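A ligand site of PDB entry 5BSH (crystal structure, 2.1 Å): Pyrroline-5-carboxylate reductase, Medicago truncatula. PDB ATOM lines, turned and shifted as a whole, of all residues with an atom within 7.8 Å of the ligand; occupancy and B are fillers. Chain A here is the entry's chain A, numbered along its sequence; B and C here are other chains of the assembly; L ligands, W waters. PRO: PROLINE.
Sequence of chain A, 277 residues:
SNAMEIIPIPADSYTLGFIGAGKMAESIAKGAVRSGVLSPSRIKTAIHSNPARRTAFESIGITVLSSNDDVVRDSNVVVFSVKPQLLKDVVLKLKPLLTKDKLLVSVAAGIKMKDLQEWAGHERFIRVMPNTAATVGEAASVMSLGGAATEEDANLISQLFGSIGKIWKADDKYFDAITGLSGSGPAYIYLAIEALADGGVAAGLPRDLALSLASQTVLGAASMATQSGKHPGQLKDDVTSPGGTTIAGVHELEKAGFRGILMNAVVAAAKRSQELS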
ATOM      1  N   ASP A 238      33.382  28.182  18.693  1.00  0.00           N
ATOM      2  CA  ASP A 238      32.766  29.270  19.499  1.00  0.00           C
ATOM      3  C   ASP A 238      31.276  29.119  19.639  1.00  0.00           C
ATOM      4  O   ASP A 238      30.739  29.524  20.641  1.00  0.00           O
ATOM      5  CB  ASP A 238      32.994  30.648  18.888  1.00  0.00           C
ATOM      6  CG  ASP A 238      34.505  31.100  18.881  1.00  0.00           C
ATOM      7  OD1 ASP A 238      35.308  30.475  19.612  1.00  0.00           O
ATOM      8  OD2 ASP A 238      34.798  32.073  18.147  1.00  0.00           O
ATOM      9  N   VAL A 239      30.571  28.516  18.678  1.00  0.00           N
ATOM     10  CA  VAL A 239      29.113  28.435  18.804  1.00  0.00           C
ATOM     11  C   VAL A 239      28.562  27.099  19.242  1.00  0.00           C
ATOM     12  O   VAL A 239      27.365  26.935  19.393  1.00  0.00           O
ATOM     13  CB  VAL A 239      28.396  28.890  17.499  1.00  0.00           C
ATOM     14  CG1 VAL A 239      28.718  30.332  17.211  1.00  0.00           C
ATOM     15  CG2 VAL A 239      28.852  28.102  16.326  1.00  0.00           C
ATOM     16  N   THR A 240      29.414  26.102  19.370  1.00  0.00           N
ATOM     17  CA  THR A 240      28.934  24.761  19.704  1.00  0.00           C
ATOM     18  C   THR A 240      28.973  24.548  21.263  1.00  0.00           C
ATOM     19  O   THR A 240      29.885  23.929  21.770  1.00  0.00           O
ATOM     20  CB  THR A 240      29.699  23.672  18.963  1.00  0.00           C
ATOM     21  OG1 THR A 240      31.114  23.968  18.910  1.00  0.00           O
ATOM     22  CG2 THR A 240      29.222  23.599  17.481  1.00  0.00           C
ATOM     23  N   SER A 241      27.924  24.990  21.956  1.00  0.00           N
ATOM     24  CA  SER A 241      27.744  24.755  23.406  1.00  0.00           C
ATOM     25  C   SER A 241      27.655  23.301  23.724  1.00  0.00           C
ATOM     26  O   SER A 241      27.049  22.538  22.965  1.00  0.00           O
ATOM     27  CB  SER A 241      26.434  25.309  23.901  1.00  0.00           C
ATOM     28  OG  SER A 241      26.208  26.567  23.330  1.00  0.00           O
ATOM     29  N   PRO A 242      28.202  22.901  24.878  1.00  0.00           N
ATOM     30  CA  PRO A 242      28.207  21.469  25.286  1.00  0.00           C
ATOM     31  C   PRO A 242      26.832  20.806  25.264  1.00  0.00           C
ATOM     32  O   PRO A 242      25.905  21.320  25.810  1.00  0.00           O
ATOM     33  CB  PRO A 242      28.711  21.518  26.740  1.00  0.00           C
ATOM     34  CG  PRO A 242      29.540  22.765  26.788  1.00  0.00           C
ATOM     35  CD  PRO A 242      28.930  23.749  25.843  1.00  0.00           C
ATOM     36  N   GLY A 243      26.683  19.721  24.500  1.00  0.00           N
ATOM     37  CA  GLY A 243      25.365  19.008  24.409  1.00  0.00           C
ATOM     38  C   GLY A 243      24.207  19.838  23.849  1.00  0.00           C
ATOM     39  O   GLY A 243      23.052  19.478  24.026  1.00  0.00           O
ATOM     40  N   GLY A 244      24.518  20.951  23.210  1.00  0.00           N
ATOM     41  CA  GLY A 244      23.485  21.898  22.809  1.00  0.00           C
ATOM     42  C   GLY A 244      22.924  21.653  21.417  1.00  0.00           C
ATOM     43  O   GLY A 244      23.191  20.651  20.753  1.00  0.00           O
ATOM     44  N   THR A 245      22.102  22.598  20.997  1.00  0.00           N
ATOM     45  CA  THR A 245      21.381  22.519  19.726  1.00  0.00           C
ATOM     46  C   THR A 245      22.322  22.580  18.530  1.00  0.00           C
ATOM     47  O   THR A 245      22.177  21.802  17.605  1.00  0.00           O
ATOM     48  CB  THR A 245      20.351  23.660  19.611  1.00  0.00           C
ATOM     49  OG1 THR A 245      21.019  24.906  19.475  1.00  0.00           O
ATOM     50  CG2 THR A 245      19.456  23.717  20.822  1.00  0.00           C
ATOM     51  N   THR A 246      23.335  23.437  18.616  1.00  0.00           N
ATOM     52  CA  THR A 246      24.293  23.622  17.482  1.00  0.00           C
ATOM     53  C   THR A 246      25.084  22.378  17.164  1.00  0.00           C
ATOM     54  O   THR A 246      25.121  21.900  15.983  1.00  0.00           O
ATOM     55  CB  THR A 246      25.150  24.842  17.706  1.00  0.00           C
ATOM     56  OG1 THR A 246      24.280  25.945  17.999  1.00  0.00           O
ATOM     57  CG2 THR A 246      25.940  25.177  16.498  1.00  0.00           C
ATOM     58  N   ILE A 247      25.588  21.740  18.201  1.00  0.00           N
ATOM     59  CA  ILE A 247      26.356  20.486  18.005  1.00  0.00           C
ATOM     60  C   ILE A 247      25.475  19.353  17.537  1.00  0.00           C
ATOM     61  O   ILE A 247      25.917  18.486  16.775  1.00  0.00           O
ATOM     62  CB  ILE A 247      27.208  20.104  19.217  1.00  0.00           C
ATOM     63  CG1 ILE A 247      28.220  19.028  18.860  1.00  0.00           C
ATOM     64  CG2 ILE A 247      26.338  19.585  20.386  1.00  0.00           C
ATOM     65  CD1 ILE A 247      29.352  19.589  18.006  1.00  0.00           C
ATOM     66  N   ALA A 248      24.215  19.346  17.956  1.00  0.00           N
ATOM     67  CA  ALA A 248      23.343  18.340  17.453  1.00  0.00           C
ATOM     68  C   ALA A 248      23.161  18.509  15.923  1.00  0.00           C
ATOM     69  O   ALA A 248      23.148  17.532  15.147  1.00  0.00           O
ATOM     70  CB  ALA A 248      21.987  18.383  18.176  1.00  0.00           C
ATOM     71  N   PRO B  84      22.093  31.036  30.449  1.00  0.00           N
ATOM     72  CA  PRO B  84      20.702  30.609  30.667  1.00  0.00           C
ATOM     73  C   PRO B  84      20.468  29.893  32.010  1.00  0.00           C
ATOM     74  O   PRO B  84      19.492  30.183  32.682  1.00  0.00           O
ATOM     75  CB  PRO B  84      20.434  29.647  29.494  1.00  0.00           C
ATOM     76  CG  PRO B  84      21.422  30.039  28.429  1.00  0.00           C
ATOM     77  CD  PRO B  84      22.579  30.723  29.082  1.00  0.00           C
ATOM     78  N   ALA B 109      19.240  32.057  25.549  1.00  0.00           N
ATOM     79  CA  ALA B 109      18.836  30.912  24.699  1.00  0.00           C
ATOM     80  C   ALA B 109      17.986  29.898  25.493  1.00  0.00           C
ATOM     81  O   ALA B 109      18.273  29.607  26.653  1.00  0.00           O
ATOM     82  CB  ALA B 109      20.069  30.215  24.115  1.00  0.00           C
ATOM     83  N   GLY B 110      16.916  29.418  24.869  1.00  0.00           N
ATOM     84  CA  GLY B 110      16.106  28.332  25.420  1.00  0.00           C
ATOM     85  C   GLY B 110      15.139  28.659  26.573  1.00  0.00           C
ATOM     86  O   GLY B 110      14.369  27.818  26.949  1.00  0.00           O
ATOM     87  N   MET B 129      15.958  36.536  20.704  1.00  0.00           N
ATOM     88  CA  MET B 129      16.914  35.518  20.402  1.00  0.00           C
ATOM     89  C   MET B 129      17.787  36.097  19.280  1.00  0.00           C
ATOM     90  O   MET B 129      17.453  35.992  18.080  1.00  0.00           O
ATOM     91  CB  MET B 129      16.239  34.234  19.991  1.00  0.00           C
ATOM     92  CG  MET B 129      17.101  33.097  19.405  1.00  0.00           C
ATOM     93  SD  MET B 129      18.158  32.437  20.703  1.00  0.00           S
ATOM     94  CE  MET B 129      19.301  31.344  19.819  1.00  0.00           C
ATOM     95  N   PRO B 130      18.964  36.587  19.643  1.00  0.00           N
ATOM     96  CA  PRO B 130      19.909  36.996  18.570  1.00  0.00           C
ATOM     97  C   PRO B 130      20.761  35.779  18.163  1.00  0.00           C
ATOM     98  O   PRO B 130      20.478  34.680  18.586  1.00  0.00           O
ATOM     99  CB  PRO B 130      20.712  38.093  19.257  1.00  0.00           C
ATOM    100  CG  PRO B 130      20.652  37.747  20.730  1.00  0.00           C
ATOM    101  CD  PRO B 130      19.543  36.739  20.968  1.00  0.00           C
ATOM    102  N   ASN B 131      21.785  35.969  17.371  1.00  0.00           N
ATOM    103  CA  ASN B 131      22.750  34.940  17.116  1.00  0.00           C
ATOM    104  C   ASN B 131      24.124  35.551  17.074  1.00  0.00           C
ATOM    105  O   ASN B 131      24.311  36.750  17.287  1.00  0.00           O
ATOM    106  CB  ASN B 131      22.378  34.190  15.796  1.00  0.00           C
ATOM    107  CG  ASN B 131      22.698  34.992  14.508  1.00  0.00           C
ATOM    108  OD1 ASN B 131      23.130  36.131  14.536  1.00  0.00           O
ATOM    109  ND2 ASN B 131      22.416  34.358  13.349  1.00  0.00           N
ATOM    110  N   THR B 132      25.104  34.722  16.852  1.00  0.00           N
ATOM    111  CA  THR B 132      26.507  35.102  17.043  1.00  0.00           C
ATOM    112  C   THR B 132      27.028  36.254  16.161  1.00  0.00           C
ATOM    113  O   THR B 132      28.021  36.905  16.461  1.00  0.00           O
ATOM    114  CB  THR B 132      27.350  33.867  16.761  1.00  0.00           C
ATOM    115  OG1 THR B 132      28.698  34.093  17.130  1.00  0.00           O
ATOM    116  CG2 THR B 132      27.339  33.544  15.212  1.00  0.00           C
ATOM    117  N   ILE B 178      13.522  28.366  15.623  1.00  0.00           N
ATOM    118  CA  ILE B 178      14.367  29.453  15.288  1.00  0.00           C
ATOM    119  C   ILE B 178      15.777  29.165  15.777  1.00  0.00           C
ATOM    120  O   ILE B 178      16.735  29.408  15.075  1.00  0.00           O
ATOM    121  CB  ILE B 178      13.840  30.781  15.870  1.00  0.00           C
ATOM    122  CG1 ILE B 178      12.536  31.134  15.146  1.00  0.00           C
ATOM    123  CG2 ILE B 178      14.855  31.886  15.746  1.00  0.00           C
ATOM    124  CD1 ILE B 178      11.670  32.174  15.872  1.00  0.00           C
ATOM    125  N   THR B 179      15.891  28.591  16.953  1.00  0.00           N
ATOM    126  CA  THR B 179      17.177  28.236  17.501  1.00  0.00           C
ATOM    127  C   THR B 179      17.955  27.271  16.596  1.00  0.00           C
ATOM    128  O   THR B 179      19.160  27.415  16.392  1.00  0.00           O
ATOM    129  CB  THR B 179      17.037  27.642  18.925  1.00  0.00           C
ATOM    130  OG1 THR B 179      16.375  28.622  19.765  1.00  0.00           O
ATOM    131  CG2 THR B 179      18.371  27.299  19.586  1.00  0.00           C
ATOM    132  N   GLY B 180      17.237  26.305  16.045  1.00  0.00           N
ATOM    133  CA  GLY B 180      17.854  25.298  15.130  1.00  0.00           C
ATOM    134  C   GLY B 180      18.286  25.918  13.811  1.00  0.00           C
ATOM    135  O   GLY B 180      19.140  25.376  13.136  1.00  0.00           O
ATOM    136  N   SER B 182      18.482  30.017  12.892  1.00  0.00           N
ATOM    137  CA  SER B 182      19.342  31.226  13.053  1.00  0.00           C
ATOM    138  C   SER B 182      20.302  31.132  14.195  1.00  0.00           C
ATOM    139  O   SER B 182      21.389  31.701  14.124  1.00  0.00           O
ATOM    140  CB  SER B 182      18.510  32.514  13.175  1.00  0.00           C
ATOM    141  OG  SER B 182      17.542  32.362  14.157  1.00  0.00           O
ATOM    142  N   GLY B 183      19.954  30.405  15.233  1.00  0.00           N
ATOM    143  CA  GLY B 183      20.854  30.239  16.386  1.00  0.00           C
ATOM    144  C   GLY B 183      22.016  29.307  16.100  1.00  0.00           C
ATOM    145  O   GLY B 183      23.200  29.635  16.354  1.00  0.00           O
ATOM    146  N   SER B 184      21.682  28.183  15.511  1.00  0.00           N
ATOM    147  CA  SER B 184      22.652  27.129  15.231  1.00  0.00           C
ATOM    148  C   SER B 184      23.222  27.189  13.871  1.00  0.00           C
ATOM    149  O   SER B 184      24.339  26.731  13.627  1.00  0.00           O
ATOM    150  CB  SER B 184      22.016  25.780  15.455  1.00  0.00           C
ATOM    151  OG  SER B 184      21.568  25.699  16.780  1.00  0.00           O
ATOM    152  N   GLY B 185      22.470  27.782  12.943  1.00  0.00           N
ATOM    153  CA  GLY B 185      22.901  27.838  11.547  1.00  0.00           C
ATOM    154  C   GLY B 185      24.335  28.359  11.276  1.00  0.00           C
ATOM    155  O   GLY B 185      24.945  27.946  10.323  1.00  0.00           O
ATOM    156  N   PRO B 186      24.830  29.312  12.050  1.00  0.00           N
ATOM    157  CA  PRO B 186      26.158  29.792  11.690  1.00  0.00           C
ATOM    158  C   PRO B 186      27.190  28.696  11.667  1.00  0.00           C
ATOM    159  O   PRO B 186      28.084  28.708  10.836  1.00  0.00           O
ATOM    160  CB  PRO B 186      26.461  30.793  12.790  1.00  0.00           C
ATOM    161  CG  PRO B 186      25.132  31.381  13.088  1.00  0.00           C
ATOM    162  CD  PRO B 186      24.186  30.233  13.005  1.00  0.00           C
ATOM    163  N   ALA B 269      18.509  20.068  15.330  1.00  0.00           N
ATOM    164  CA  ALA B 269      18.803  21.137  16.242  1.00  0.00           C
ATOM    165  C   ALA B 269      17.550  21.656  16.919  1.00  0.00           C
ATOM    166  O   ALA B 269      17.570  21.936  18.114  1.00  0.00           O
ATOM    167  CB  ALA B 269      19.559  22.255  15.547  1.00  0.00           C
ATOM    168  N   ARG B 272      16.512  19.182  19.483  1.00  0.00           N
ATOM    169  CA  ARG B 272      17.352  19.244  20.681  1.00  0.00           C
ATOM    170  C   ARG B 272      16.971  20.445  21.525  1.00  0.00           C
ATOM    171  O   ARG B 272      16.957  20.374  22.762  1.00  0.00           O
ATOM    172  CB  ARG B 272      18.812  19.324  20.323  1.00  0.00           C
ATOM    173  CG  ARG B 272      19.738  19.391  21.519  1.00  0.00           C
ATOM    174  CD  ARG B 272      19.567  18.185  22.442  1.00  0.00           C
ATOM    175  NE  ARG B 272      20.661  18.148  23.406  1.00  0.00           N
ATOM    176  CZ  ARG B 272      20.619  17.557  24.590  1.00  0.00           C
ATOM    177  NH1 ARG B 272      19.475  16.944  24.994  1.00  0.00           N
ATOM    178  NH2 ARG B 272      21.703  17.590  25.381  1.00  0.00           N
ATOM    179  N   SER B 273      16.632  21.551  20.883  1.00  0.00           N
ATOM    180  CA  SER B 273      16.211  22.767  21.602  1.00  0.00           C
ATOM    181  C   SER B 273      14.962  22.505  22.401  1.00  0.00           C
ATOM    182  O   SER B 273      14.845  22.824  23.576  1.00  0.00           O
ATOM    183  CB  SER B 273      15.957  23.900  20.635  1.00  0.00           C
ATOM    184  OG  SER B 273      15.440  25.024  21.269  1.00  0.00           O
ATOM    185  N   LEU B 276      15.801  20.311  25.470  1.00  0.00           N
ATOM    186  CA  LEU B 276      16.529  20.995  26.536  1.00  0.00           C
ATOM    187  C   LEU B 276      15.534  21.853  27.260  1.00  0.00           C
ATOM    188  O   LEU B 276      15.887  22.670  28.057  1.00  0.00           O
ATOM    189  CB  LEU B 276      17.691  21.833  25.966  1.00  0.00           C
ATOM    190  CG  LEU B 276      18.843  20.934  25.528  1.00  0.00           C
ATOM    191  CD1 LEU B 276      19.860  21.743  24.730  1.00  0.00           C
ATOM    192  CD2 LEU B 276      19.495  20.232  26.721  1.00  0.00           C
ATOM    193  N   VAL C 201      31.882  17.060  22.777  1.00  0.00           N
ATOM    194  CA  VAL C 201      30.920  18.159  22.912  1.00  0.00           C
ATOM    195  C   VAL C 201      29.493  17.664  22.599  1.00  0.00           C
ATOM    196  O   VAL C 201      28.525  18.063  23.253  1.00  0.00           O
ATOM    197  CB  VAL C 201      31.313  19.340  22.005  1.00  0.00           C
ATOM    198  CG1 VAL C 201      30.283  20.443  22.013  1.00  0.00           C
ATOM    199  CG2 VAL C 201      32.644  19.916  22.399  1.00  0.00           C
HETATM  200  N   PRO L   1      24.348  28.155  20.392  1.00  0.00           N
HETATM  201  CA  PRO L   1      23.607  27.552  21.508  1.00  0.00           C
HETATM  202  C   PRO L   1      23.716  26.042  21.510  1.00  0.00           C
HETATM  203  O   PRO L   1      22.748  25.413  22.052  1.00  0.00           O
HETATM  204  CB  PRO L   1      22.163  27.978  21.229  1.00  0.00           C
HETATM  205  CG  PRO L   1      22.132  28.453  19.821  1.00  0.00           C
HETATM  206  CD  PRO L   1      23.487  29.016  19.575  1.00  0.00           C
HETATM  207  OXT PRO L   1      24.749  25.535  20.972  1.00  0.00           O
HETATM  208  O   HOH W   1      25.702  23.147  20.637  1.00  0.00           O
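The backbone NH of Ser 241 lies within hydrogen-bond range of an oxygen (OXT) of the ligand, at 3.4 Å. The side-chain hydroxyl of Ser 241 is in hydrogen-bond range of an oxygen (OXT) of the ligand, 3.0 Å away. An oxygen (OXT) of the ligand sits close to the backbone NH (N) of Thr 246 (3.5 Å). An oxygen (OXT) of the ligand sits at hydrogen-bond distance from the side-chain hydroxyl of Thr 246 (3.0 Å). N of Thr 245 is in hydrogen-bond range of O of the ligand, at 3.1 Å. The side-chain hydroxyl of Thr 245 is in hydrogen-bond range of an oxygen (O) of the ligand, 3.1 Å away. The backbone carbonyl oxygen of Val 239 sits at hydrogen-bond distance from a nitrogen (N) of the ligand.
OG of Ser 184 of chain B lies within hydrogen-bond range of OG1 of Thr 246, at 3.0 Å. OG1 of Thr 245 is in hydrogen-bond range of OG of Ser 184 of chain B. N of Gly 183 of chain B is in hydrogen-bond range of O of Ile 178 of chain B (3.4 Å). O of Thr 179 of chain B sits at hydrogen-bond distance from N of Ser 184 of chain B, 2.8 Å away.
Gly 244 touches the ligand (CA to O, 3.7 Å). Thr 179 of chain B touches the ligand. Gly 183 of chain B touches the ligand (O to CD, 3.3 Å). Within 4 Å of the ligand: Val 239, Ser 241, Gly 244, Thr 245, Thr 246, Thr 179 of chain B and Gly 183 of chain B.
Water W1 lies within hydrogen-bond range of an oxygen (OXT) of the ligand (2.6 Å), the backbone carbonyl oxygen of Ser 241 (2.8 Å), the backbone NH of Ile 247 (2.8 Å) and the backbone NH of Thr 246 (3.1 Å).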
